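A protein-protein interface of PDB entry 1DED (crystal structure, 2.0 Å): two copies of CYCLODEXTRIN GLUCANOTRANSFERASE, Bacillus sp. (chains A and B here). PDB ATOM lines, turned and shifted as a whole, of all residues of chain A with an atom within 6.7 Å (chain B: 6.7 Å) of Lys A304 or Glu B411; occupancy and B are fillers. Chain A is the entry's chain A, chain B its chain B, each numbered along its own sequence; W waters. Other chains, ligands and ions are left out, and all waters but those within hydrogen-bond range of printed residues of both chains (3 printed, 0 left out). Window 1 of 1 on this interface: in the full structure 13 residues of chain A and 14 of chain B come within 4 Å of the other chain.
The side-chain hydroxyl (OH) of Tyr A301 lies within hydrogen-bond range of the backbone carbonyl oxygen (O) of Ile B414. The side-chain amino group (NZ) of Lys A304 is in salt-bridge range of the side-chain carboxylate (OE1) of Glu B411 (3.9 Å). The side-chain carboxylate (OE2) of Glu A411 lies within salt-bridge range of the side-chain amino group (NZ) of Lys B304. O of Ile A414 is in hydrogen-bond range of OH of Tyr B301 (2.9 Å). The side-chain carboxylate of Glu B411 lies close to the side-chain carboxylate of Glu A411 (2.8 Å).
Tyr A301 touches Arg B412, but with the chains exchanged Arg A412 does not touch Tyr B301 (4.8 Å). Tyr A301 touches Ile B414, and with the chains exchanged Ile A414 touches Tyr B301. Lys A304 touches Arg B412, and with the chains exchanged Arg A412 touches Lys B304. Glu A411 touches its own counterpart, Glu B411. 8 positions are printed for both chains.
Among the printed residues, merely in contact across the chains: Arg A412 with Lys B304 (3.2 Å), Tyr A301 with Trp B413 (3.4 Å), Lys A304 with Arg B412 (3.5 Å), Trp A413 with Tyr B301 (3.6 Å), Ile A414 with Ile B414 (3.8 Å) and Tyr A301 with Arg B412 (3.9 Å).
Of the printed residues of chain B, Lys A304 touches Glu B411 (3.1 Å) and Arg B412 (3.5 Å). Glu A308 touches none of the printed residues of chain B. Of the printed residues of chain A, Lys B304 touches Glu A411 (3.0 Å) and Arg A412 (3.2 Å). Of the printed residues of chain A, Ile B414 touches Tyr A301 (2.9 Å) and Ile A414 (3.8 Å). The nearest residue of chain B that does not touch Lys A304 is Trp B413 (4.9 Å). The nearest printed residue of chain B that does not touch Trp A413 is Lys B304 (4.5 Å).
The side-chain amide oxygen of Asn A299 lies within hydrogen-bond range of the backbone NH of Tyr A301. NZ of Lys A304 lies within salt-bridge range of OE1 of Glu A411 (3.0 Å). The side-chain carboxylate (OE2) of Glu A411 sits at hydrogen-bond distance from the backbone NH (N) of Trp A413 (3.1 Å). NZ of Lys B304 is in salt-bridge range of OE1 of Glu B308, 2.9 Å away. The side-chain amino group of Lys B304 is in salt-bridge range of the side-chain carboxylate of Glu B411 (3.1 Å). The side-chain carboxylate of Glu B422 is in salt-bridge range of the guanidinium group of Arg B412 (3.1 Å).
Water W2 bridges the side-chain carboxylate of Glu A308 (2.8 Å) and the guanidinium group of Arg B412 (3.3 Å). Water W1 bridges NH1 of Arg A412 and OE2 of Glu B308. Water W3 lies within hydrogen-bond range of OH of Tyr A301 and O of Ile B414.
Printed residues of chain A that touch a printed residue of chain B: Tyr A301, Lys A304, Glu A411, Arg A412, Trp A413 and Ile A414. Printed residues of chain B that touch a printed residue of chain A: Tyr B301, Lys B304, Glu B411, Arg B412, Trp B413 and Ile B414. Hydrophobic or aromatic side chains of chain B that line the printed part of chain A: Tyr B301, Trp B413 and Ile B414.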
ATOM      1  N   LYS A 288       8.001  28.448  -3.755  1.00  0.00           N
ATOM      2  CA  LYS A 288       7.313  28.890  -2.551  1.00  0.00           C
ATOM      3  C   LYS A 288       7.834  30.238  -2.063  1.00  0.00           C
ATOM      4  O   LYS A 288       7.071  31.031  -1.503  1.00  0.00           O
ATOM      5  CB  LYS A 288       7.454  27.833  -1.427  1.00  0.00           C
ATOM      6  CG  LYS A 288       6.684  28.089  -0.137  1.00  0.00           C
ATOM      7  CD  LYS A 288       5.177  28.076  -0.296  1.00  0.00           C
ATOM      8  CE  LYS A 288       4.731  26.739  -0.908  1.00  0.00           C
ATOM      9  NZ  LYS A 288       3.303  26.746  -1.138  1.00  0.00           N
ATOM     10  N   ASN A 299       1.534  32.207   2.654  1.00  0.00           N
ATOM     11  CA  ASN A 299       2.044  32.970   3.774  1.00  0.00           C
ATOM     12  C   ASN A 299       3.194  32.305   4.482  1.00  0.00           C
ATOM     13  O   ASN A 299       3.746  31.334   3.964  1.00  0.00           O
ATOM     14  CB  ASN A 299       0.897  33.249   4.767  1.00  0.00           C
ATOM     15  CG  ASN A 299       0.277  32.029   5.440  1.00  0.00           C
ATOM     16  OD1 ASN A 299       0.901  30.988   5.626  1.00  0.00           O
ATOM     17  ND2 ASN A 299      -0.978  32.113   5.837  1.00  0.00           N
ATOM     18  N   MET A 300       3.572  32.766   5.678  1.00  0.00           N
ATOM     19  CA  MET A 300       4.733  32.196   6.324  1.00  0.00           C
ATOM     20  C   MET A 300       4.603  30.770   6.749  1.00  0.00           C
ATOM     21  O   MET A 300       5.630  30.107   6.856  1.00  0.00           O
ATOM     22  CB  MET A 300       5.140  33.025   7.541  1.00  0.00           C
ATOM     23  CG  MET A 300       5.731  34.350   7.110  1.00  0.00           C
ATOM     24  SD  MET A 300       7.172  34.220   6.020  1.00  0.00           S
ATOM     25  CE  MET A 300       7.419  35.932   5.651  1.00  0.00           C
ATOM     26  N   TYR A 301       3.376  30.278   6.921  1.00  0.00           N
ATOM     27  CA  TYR A 301       3.120  28.887   7.311  1.00  0.00           C
ATOM     28  C   TYR A 301       3.437  27.918   6.192  1.00  0.00           C
ATOM     29  O   TYR A 301       4.055  26.874   6.406  1.00  0.00           O
ATOM     30  CB  TYR A 301       1.663  28.718   7.748  1.00  0.00           C
ATOM     31  CG  TYR A 301       1.499  29.215   9.181  1.00  0.00           C
ATOM     32  CD1 TYR A 301       0.749  30.358   9.448  1.00  0.00           C
ATOM     33  CD2 TYR A 301       2.152  28.533  10.211  1.00  0.00           C
ATOM     34  CE1 TYR A 301       0.666  30.823  10.757  1.00  0.00           C
ATOM     35  CE2 TYR A 301       2.070  28.989  11.518  1.00  0.00           C
ATOM     36  CZ  TYR A 301       1.330  30.127  11.771  1.00  0.00           C
ATOM     37  OH  TYR A 301       1.253  30.558  13.065  1.00  0.00           O
ATOM     38  N   GLY A 302       3.122  28.416   4.986  1.00  0.00           N
ATOM     39  CA  GLY A 302       3.516  27.777   3.747  1.00  0.00           C
ATOM     40  C   GLY A 302       5.031  27.768   3.618  1.00  0.00           C
ATOM     41  O   GLY A 302       5.622  26.771   3.191  1.00  0.00           O
ATOM     42  N   LEU A 303       5.678  28.886   3.964  1.00  0.00           N
ATOM     43  CA  LEU A 303       7.130  28.987   3.940  1.00  0.00           C
ATOM     44  C   LEU A 303       7.728  27.964   4.907  1.00  0.00           C
ATOM     45  O   LEU A 303       8.570  27.167   4.524  1.00  0.00           O
ATOM     46  CB  LEU A 303       7.564  30.393   4.356  1.00  0.00           C
ATOM     47  CG  LEU A 303       9.005  30.753   4.047  1.00  0.00           C
ATOM     48  CD1 LEU A 303       9.088  31.191   2.605  1.00  0.00           C
ATOM     49  CD2 LEU A 303       9.474  31.911   4.900  1.00  0.00           C
ATOM     50  N   LYS A 304       7.299  27.940   6.157  1.00  0.00           N
ATOM     51  CA  LYS A 304       7.714  26.996   7.201  1.00  0.00           C
ATOM     52  C   LYS A 304       7.511  25.545   6.749  1.00  0.00           C
ATOM     53  O   LYS A 304       8.473  24.763   6.749  1.00  0.00           O
ATOM     54  CB  LYS A 304       6.882  27.311   8.461  1.00  0.00           C
ATOM     55  CG  LYS A 304       6.848  26.312   9.623  1.00  0.00           C
ATOM     56  CD  LYS A 304       5.773  26.720  10.636  1.00  0.00           C
ATOM     57  CE  LYS A 304       5.423  25.606  11.636  1.00  0.00           C
ATOM     58  NZ  LYS A 304       6.602  25.084  12.324  1.00  0.00           N
ATOM     59  N   ALA A 305       6.300  25.193   6.296  1.00  0.00           N
ATOM     60  CA  ALA A 305       5.995  23.828   5.865  1.00  0.00           C
ATOM     61  C   ALA A 305       6.940  23.391   4.759  1.00  0.00           C
ATOM     62  O   ALA A 305       7.459  22.275   4.806  1.00  0.00           O
ATOM     63  CB  ALA A 305       4.569  23.753   5.360  1.00  0.00           C
ATOM     64  N   MET A 306       7.270  24.258   3.793  1.00  0.00           N
ATOM     65  CA  MET A 306       8.241  23.927   2.753  1.00  0.00           C
ATOM     66  C   MET A 306       9.639  23.758   3.340  1.00  0.00           C
ATOM     67  O   MET A 306      10.361  22.835   2.927  1.00  0.00           O
ATOM     68  CB  MET A 306       8.270  25.029   1.679  1.00  0.00           C
ATOM     69  CG  MET A 306       9.303  24.952   0.547  1.00  0.00           C
ATOM     70  SD  MET A 306      10.980  25.428   1.016  1.00  0.00           S
ATOM     71  CE  MET A 306      10.774  27.188   0.985  1.00  0.00           C
ATOM     72  N   LEU A 307      10.101  24.568   4.299  1.00  0.00           N
ATOM     73  CA  LEU A 307      11.476  24.375   4.764  1.00  0.00           C
ATOM     74  C   LEU A 307      11.593  23.123   5.613  1.00  0.00           C
ATOM     75  O   LEU A 307      12.627  22.454   5.624  1.00  0.00           O
ATOM     76  CB  LEU A 307      12.002  25.482   5.638  1.00  0.00           C
ATOM     77  CG  LEU A 307      12.501  26.859   5.303  1.00  0.00           C
ATOM     78  CD1 LEU A 307      13.257  26.901   3.986  1.00  0.00           C
ATOM     79  CD2 LEU A 307      11.315  27.749   5.442  1.00  0.00           C
ATOM     80  N   GLU A 308      10.521  22.826   6.336  1.00  0.00           N
ATOM     81  CA  GLU A 308      10.494  21.673   7.209  1.00  0.00           C
ATOM     82  C   GLU A 308      10.354  20.404   6.409  1.00  0.00           C
ATOM     83  O   GLU A 308      11.145  19.477   6.569  1.00  0.00           O
ATOM     84  CB  GLU A 308       9.358  21.828   8.178  1.00  0.00           C
ATOM     85  CG  GLU A 308       9.856  22.701   9.335  1.00  0.00           C
ATOM     86  CD  GLU A 308       8.785  23.196  10.305  1.00  0.00           C
ATOM     87  OE1 GLU A 308       9.111  24.057  11.127  1.00  0.00           O
ATOM     88  OE2 GLU A 308       7.635  22.746  10.251  1.00  0.00           O
ATOM     89  N   GLY A 309       9.422  20.415   5.478  1.00  0.00           N
ATOM     90  CA  GLY A 309       9.217  19.294   4.594  1.00  0.00           C
ATOM     91  C   GLY A 309      10.438  18.978   3.766  1.00  0.00           C
ATOM     92  O   GLY A 309      10.862  17.828   3.666  1.00  0.00           O
ATOM     93  N   SER A 310      11.092  19.980   3.188  1.00  0.00           N
ATOM     94  CA  SER A 310      12.189  19.695   2.293  1.00  0.00           C
ATOM     95  C   SER A 310      13.407  19.191   3.014  1.00  0.00           C
ATOM     96  O   SER A 310      14.216  18.493   2.402  1.00  0.00           O
ATOM     97  CB  SER A 310      12.553  20.926   1.490  1.00  0.00           C
ATOM     98  OG  SER A 310      12.878  22.008   2.330  1.00  0.00           O
ATOM     99  N   GLU A 411      12.247  26.866  13.081  1.00  0.00           N
ATOM    100  CA  GLU A 411      11.447  28.062  13.197  1.00  0.00           C
ATOM    101  C   GLU A 411      11.246  28.438  14.665  1.00  0.00           C
ATOM    102  O   GLU A 411      10.619  27.692  15.417  1.00  0.00           O
ATOM    103  CB  GLU A 411      10.108  27.852  12.494  1.00  0.00           C
ATOM    104  CG  GLU A 411       9.012  28.909  12.694  1.00  0.00           C
ATOM    105  CD  GLU A 411       8.091  28.581  13.852  1.00  0.00           C
ATOM    106  OE1 GLU A 411       7.304  27.664  13.692  1.00  0.00           O
ATOM    107  OE2 GLU A 411       8.133  29.213  14.910  1.00  0.00           O
ATOM    108  N   ARG A 412      11.781  29.588  15.094  1.00  0.00           N
ATOM    109  CA  ARG A 412      11.631  30.062  16.458  1.00  0.00           C
ATOM    110  C   ARG A 412      10.431  30.962  16.660  1.00  0.00           C
ATOM    111  O   ARG A 412       9.917  31.026  17.786  1.00  0.00           O
ATOM    112  CB  ARG A 412      12.852  30.822  16.896  1.00  0.00           C
ATOM    113  CG  ARG A 412      14.118  29.997  17.037  1.00  0.00           C
ATOM    114  CD  ARG A 412      13.879  28.896  18.034  1.00  0.00           C
ATOM    115  NE  ARG A 412      15.164  28.378  18.441  1.00  0.00           N
ATOM    116  CZ  ARG A 412      15.335  27.758  19.608  1.00  0.00           C
ATOM    117  NH1 ARG A 412      14.330  27.567  20.478  1.00  0.00           N
ATOM    118  NH2 ARG A 412      16.559  27.352  19.925  1.00  0.00           N
ATOM    119  N   TRP A 413       9.912  31.690  15.662  1.00  0.00           N
ATOM    120  CA  TRP A 413       8.722  32.526  15.873  1.00  0.00           C
ATOM    121  C   TRP A 413       8.014  32.654  14.539  1.00  0.00           C
ATOM    122  O   TRP A 413       8.700  32.635  13.514  1.00  0.00           O
ATOM    123  CB  TRP A 413       9.137  33.938  16.403  1.00  0.00           C
ATOM    124  CG  TRP A 413       8.067  34.722  17.159  1.00  0.00           C
ATOM    125  CD1 TRP A 413       7.960  34.637  18.531  1.00  0.00           C
ATOM    126  CD2 TRP A 413       7.099  35.555  16.613  1.00  0.00           C
ATOM    127  NE1 TRP A 413       6.931  35.402  18.859  1.00  0.00           N
ATOM    128  CE2 TRP A 413       6.391  35.962  17.752  1.00  0.00           C
ATOM    129  CE3 TRP A 413       6.720  36.001  15.348  1.00  0.00           C
ATOM    130  CZ2 TRP A 413       5.297  36.817  17.634  1.00  0.00           C
ATOM    131  CZ3 TRP A 413       5.623  36.854  15.233  1.00  0.00           C
ATOM    132  CH2 TRP A 413       4.916  37.260  16.367  1.00  0.00           C
ATOM    133  N   ILE A 414       6.700  32.852  14.487  1.00  0.00           N
ATOM    134  CA  ILE A 414       5.988  32.934  13.230  1.00  0.00           C
ATOM    135  C   ILE A 414       4.614  33.532  13.465  1.00  0.00           C
ATOM    136  O   ILE A 414       4.095  33.512  14.582  1.00  0.00           O
ATOM    137  CB  ILE A 414       5.846  31.495  12.591  1.00  0.00           C
ATOM    138  CG1 ILE A 414       5.251  31.537  11.189  1.00  0.00           C
ATOM    139  CG2 ILE A 414       4.919  30.642  13.483  1.00  0.00           C
ATOM    140  CD1 ILE A 414       6.000  30.527  10.377  1.00  0.00           C
ATOM    141  N   ILE A 419       8.497  35.363  10.045  1.00  0.00           N
ATOM    142  CA  ILE A 419       9.085  34.105  10.430  1.00  0.00           C
ATOM    143  C   ILE A 419      10.441  34.504  10.985  1.00  0.00           C
ATOM    144  O   ILE A 419      11.091  35.401  10.438  1.00  0.00           O
ATOM    145  CB  ILE A 419       9.247  33.063   9.211  1.00  0.00           C
ATOM    146  CG1 ILE A 419       9.674  31.695   9.796  1.00  0.00           C
ATOM    147  CG2 ILE A 419      10.246  33.553   8.153  1.00  0.00           C
ATOM    148  CD1 ILE A 419       9.980  30.601   8.760  1.00  0.00           C
ATOM    149  N   TYR B 301       4.010  30.750  23.112  1.00  0.00           N
ATOM    150  CA  TYR B 301       5.393  30.702  22.642  1.00  0.00           C
ATOM    151  C   TYR B 301       6.306  30.225  23.753  1.00  0.00           C
ATOM    152  O   TYR B 301       7.354  29.625  23.504  1.00  0.00           O
ATOM    153  CB  TYR B 301       5.844  32.079  22.148  1.00  0.00           C
ATOM    154  CG  TYR B 301       5.151  32.495  20.854  1.00  0.00           C
ATOM    155  CD1 TYR B 301       4.027  33.321  20.915  1.00  0.00           C
ATOM    156  CD2 TYR B 301       5.635  32.049  19.615  1.00  0.00           C
ATOM    157  CE1 TYR B 301       3.387  33.698  19.734  1.00  0.00           C
ATOM    158  CE2 TYR B 301       4.990  32.427  18.429  1.00  0.00           C
ATOM    159  CZ  TYR B 301       3.866  33.250  18.491  1.00  0.00           C
ATOM    160  OH  TYR B 301       3.182  33.638  17.334  1.00  0.00           O
ATOM    161  N   LYS B 304       5.766  26.483  23.763  1.00  0.00           N
ATOM    162  CA  LYS B 304       6.553  26.096  22.600  1.00  0.00           C
ATOM    163  C   LYS B 304       8.012  26.017  22.962  1.00  0.00           C
ATOM    164  O   LYS B 304       8.658  25.021  22.634  1.00  0.00           O
ATOM    165  CB  LYS B 304       6.377  27.118  21.455  1.00  0.00           C
ATOM    166  CG  LYS B 304       7.342  27.058  20.259  1.00  0.00           C
ATOM    167  CD  LYS B 304       6.998  28.138  19.230  1.00  0.00           C
ATOM    168  CE  LYS B 304       8.130  28.443  18.270  1.00  0.00           C
ATOM    169  NZ  LYS B 304       8.633  27.278  17.570  1.00  0.00           N
ATOM    170  N   GLU B 308      10.268  22.517  22.907  1.00  0.00           N
ATOM    171  CA  GLU B 308      11.436  22.437  22.041  1.00  0.00           C
ATOM    172  C   GLU B 308      12.736  22.243  22.800  1.00  0.00           C
ATOM    173  O   GLU B 308      13.546  21.368  22.465  1.00  0.00           O
ATOM    174  CB  GLU B 308      11.540  23.709  21.181  1.00  0.00           C
ATOM    175  CG  GLU B 308      10.775  23.471  19.908  1.00  0.00           C
ATOM    176  CD  GLU B 308      10.278  24.686  19.137  1.00  0.00           C
ATOM    177  OE1 GLU B 308       9.260  24.543  18.436  1.00  0.00           O
ATOM    178  OE2 GLU B 308      10.904  25.752  19.233  1.00  0.00           O
ATOM    179  N   THR B 409       7.804  15.907  19.224  1.00  0.00           N
ATOM    180  CA  THR B 409       6.786  16.946  19.264  1.00  0.00           C
ATOM    181  C   THR B 409       7.228  18.004  18.263  1.00  0.00           C
ATOM    182  O   THR B 409       8.445  18.245  18.162  1.00  0.00           O
ATOM    183  CB  THR B 409       6.722  17.514  20.664  1.00  0.00           C
ATOM    184  OG1 THR B 409       6.718  16.410  21.563  1.00  0.00           O
ATOM    185  CG2 THR B 409       5.472  18.364  20.871  1.00  0.00           C
ATOM    186  N   HIS B 410       6.323  18.571  17.449  1.00  0.00           N
ATOM    187  CA  HIS B 410       6.690  19.580  16.444  1.00  0.00           C
ATOM    188  C   HIS B 410       5.540  20.543  16.355  1.00  0.00           C
ATOM    189  O   HIS B 410       4.430  20.115  16.037  1.00  0.00           O
ATOM    190  CB  HIS B 410       6.839  19.064  15.035  1.00  0.00           C
ATOM    191  CG  HIS B 410       7.253  17.614  14.896  1.00  0.00           C
ATOM    192  ND1 HIS B 410       6.440  16.565  15.055  1.00  0.00           N
ATOM    193  CD2 HIS B 410       8.526  17.158  14.616  1.00  0.00           C
ATOM    194  CE1 HIS B 410       7.170  15.502  14.890  1.00  0.00           C
ATOM    195  NE2 HIS B 410       8.413  15.851  14.630  1.00  0.00           N
ATOM    196  N   GLU B 411       5.742  21.818  16.702  1.00  0.00           N
ATOM    197  CA  GLU B 411       4.678  22.793  16.606  1.00  0.00           C
ATOM    198  C   GLU B 411       4.382  23.036  15.120  1.00  0.00           C
ATOM    199  O   GLU B 411       5.277  23.146  14.277  1.00  0.00           O
ATOM    200  CB  GLU B 411       5.164  24.039  17.366  1.00  0.00           C
ATOM    201  CG  GLU B 411       4.411  25.350  17.120  1.00  0.00           C
ATOM    202  CD  GLU B 411       4.952  26.204  15.959  1.00  0.00           C
ATOM    203  OE1 GLU B 411       6.137  26.525  15.927  1.00  0.00           O
ATOM    204  OE2 GLU B 411       4.181  26.568  15.087  1.00  0.00           O
ATOM    205  N   ARG B 412       3.115  23.121  14.792  1.00  0.00           N
ATOM    206  CA  ARG B 412       2.704  23.279  13.416  1.00  0.00           C
ATOM    207  C   ARG B 412       1.970  24.579  13.209  1.00  0.00           C
ATOM    208  O   ARG B 412       2.010  25.159  12.125  1.00  0.00           O
ATOM    209  CB  ARG B 412       1.779  22.137  13.002  1.00  0.00           C
ATOM    210  CG  ARG B 412       2.416  20.764  12.960  1.00  0.00           C
ATOM    211  CD  ARG B 412       3.425  20.854  11.868  1.00  0.00           C
ATOM    212  NE  ARG B 412       3.811  19.546  11.400  1.00  0.00           N
ATOM    213  CZ  ARG B 412       3.794  19.245  10.090  1.00  0.00           C
ATOM    214  NH1 ARG B 412       3.422  20.126   9.145  1.00  0.00           N
ATOM    215  NH2 ARG B 412       4.167  18.022   9.706  1.00  0.00           N
ATOM    216  N   TRP B 413       1.247  25.036  14.213  1.00  0.00           N
ATOM    217  CA  TRP B 413       0.576  26.317  14.132  1.00  0.00           C
ATOM    218  C   TRP B 413       0.694  26.923  15.513  1.00  0.00           C
ATOM    219  O   TRP B 413       0.674  26.165  16.495  1.00  0.00           O
ATOM    220  CB  TRP B 413      -0.889  26.159  13.789  1.00  0.00           C
ATOM    221  CG  TRP B 413      -1.460  27.410  13.130  1.00  0.00           C
ATOM    222  CD1 TRP B 413      -1.271  27.574  11.785  1.00  0.00           C
ATOM    223  CD2 TRP B 413      -2.210  28.426  13.713  1.00  0.00           C
ATOM    224  NE1 TRP B 413      -1.910  28.679  11.498  1.00  0.00           N
ATOM    225  CE2 TRP B 413      -2.482  29.222  12.595  1.00  0.00           C
ATOM    226  CE3 TRP B 413      -2.711  28.818  14.968  1.00  0.00           C
ATOM    227  CZ2 TRP B 413      -3.243  30.392  12.709  1.00  0.00           C
ATOM    228  CZ3 TRP B 413      -3.471  29.991  15.087  1.00  0.00           C
ATOM    229  CH2 TRP B 413      -3.737  30.769  13.962  1.00  0.00           C
ATOM    230  N   ILE B 414       0.852  28.246  15.625  1.00  0.00           N
ATOM    231  CA  ILE B 414       0.922  28.878  16.921  1.00  0.00           C
ATOM    232  C   ILE B 414       0.592  30.367  16.864  1.00  0.00           C
ATOM    233  O   ILE B 414       0.526  30.996  15.803  1.00  0.00           O
ATOM    234  CB  ILE B 414       2.346  28.640  17.508  1.00  0.00           C
ATOM    235  CG1 ILE B 414       2.290  28.801  19.013  1.00  0.00           C
ATOM    236  CG2 ILE B 414       3.355  29.532  16.801  1.00  0.00           C
ATOM    237  CD1 ILE B 414       3.656  28.759  19.647  1.00  0.00           C
ATOM    238  N   ASN B 415       0.265  30.872  18.052  1.00  0.00           N
ATOM    239  CA  ASN B 415       0.097  32.279  18.306  1.00  0.00           C
ATOM    240  C   ASN B 415      -0.009  32.411  19.829  1.00  0.00           C
ATOM    241  O   ASN B 415      -0.066  31.419  20.536  1.00  0.00           O
ATOM    242  CB  ASN B 415      -1.165  32.804  17.611  1.00  0.00           C
ATOM    243  CG  ASN B 415      -2.551  32.570  18.217  1.00  0.00           C
ATOM    244  OD1 ASN B 415      -3.540  32.965  17.615  1.00  0.00           O
ATOM    245  ND2 ASN B 415      -2.861  31.971  19.351  1.00  0.00           N
ATOM    246  N   ILE B 419      -1.975  26.638  20.378  1.00  0.00           N
ATOM    247  CA  ILE B 419      -0.876  25.823  19.881  1.00  0.00           C
ATOM    248  C   ILE B 419      -1.552  24.606  19.238  1.00  0.00           C
ATOM    249  O   ILE B 419      -2.629  24.172  19.679  1.00  0.00           O
ATOM    250  CB  ILE B 419       0.132  25.354  21.026  1.00  0.00           C
ATOM    251  CG1 ILE B 419       1.368  24.753  20.321  1.00  0.00           C
ATOM    252  CG2 ILE B 419      -0.502  24.378  22.012  1.00  0.00           C
ATOM    253  CD1 ILE B 419       2.599  24.317  21.157  1.00  0.00           C
ATOM    254  N   ILE B 420      -1.049  24.152  18.089  1.00  0.00           N
ATOM    255  CA  ILE B 420      -1.441  22.862  17.586  1.00  0.00           C
ATOM    256  C   ILE B 420      -0.065  22.282  17.242  1.00  0.00           C
ATOM    257  O   ILE B 420       0.798  22.875  16.572  1.00  0.00           O
ATOM    258  CB  ILE B 420      -2.496  22.915  16.339  1.00  0.00           C
ATOM    259  CG1 ILE B 420      -1.868  22.324  15.119  1.00  0.00           C
ATOM    260  CG2 ILE B 420      -3.058  24.287  16.072  1.00  0.00           C
ATOM    261  CD1 ILE B 420      -2.255  20.825  15.049  1.00  0.00           C
ATOM    262  N   TYR B 421       0.189  21.142  17.896  1.00  0.00           N
ATOM    263  CA  TYR B 421       1.439  20.403  17.777  1.00  0.00           C
ATOM    264  C   TYR B 421       1.137  19.020  17.250  1.00  0.00           C
ATOM    265  O   TYR B 421      -0.004  18.541  17.299  1.00  0.00           O
ATOM    266  CB  TYR B 421       2.185  20.261  19.130  1.00  0.00           C
ATOM    267  CG  TYR B 421       1.385  19.780  20.332  1.00  0.00           C
ATOM    268  CD1 TYR B 421       0.470  20.648  20.930  1.00  0.00           C
ATOM    269  CD2 TYR B 421       1.559  18.491  20.834  1.00  0.00           C
ATOM    270  CE1 TYR B 421      -0.279  20.253  22.021  1.00  0.00           C
ATOM    271  CE2 TYR B 421       0.806  18.081  21.939  1.00  0.00           C
ATOM    272  CZ  TYR B 421      -0.111  18.959  22.522  1.00  0.00           C
ATOM    273  OH  TYR B 421      -0.930  18.558  23.564  1.00  0.00           O
ATOM    274  N   GLU B 422       2.173  18.398  16.736  1.00  0.00           N
ATOM    275  CA  GLU B 422       2.003  17.102  16.166  1.00  0.00           C
ATOM    276  C   GLU B 422       3.063  16.222  16.755  1.00  0.00           C
ATOM    277  O   GLU B 422       4.247  16.584  16.834  1.00  0.00           O
ATOM    278  CB  GLU B 422       2.150  17.239  14.673  1.00  0.00           C
ATOM    279  CG  GLU B 422       2.173  15.970  13.876  1.00  0.00           C
ATOM    280  CD  GLU B 422       2.431  16.261  12.408  1.00  0.00           C
ATOM    281  OE1 GLU B 422       1.494  16.755  11.779  1.00  0.00           O
ATOM    282  OE2 GLU B 422       3.545  15.998  11.915  1.00  0.00           O
HETATM  283  O   HOH W   1      11.580  27.827  21.084  1.00  0.00           O
HETATM  284  O   HOH W   2       5.027  22.980   9.266  1.00  0.00           O
HETATM  285  O   HOH W   3      -0.702  32.564  13.490  1.00  0.00           O
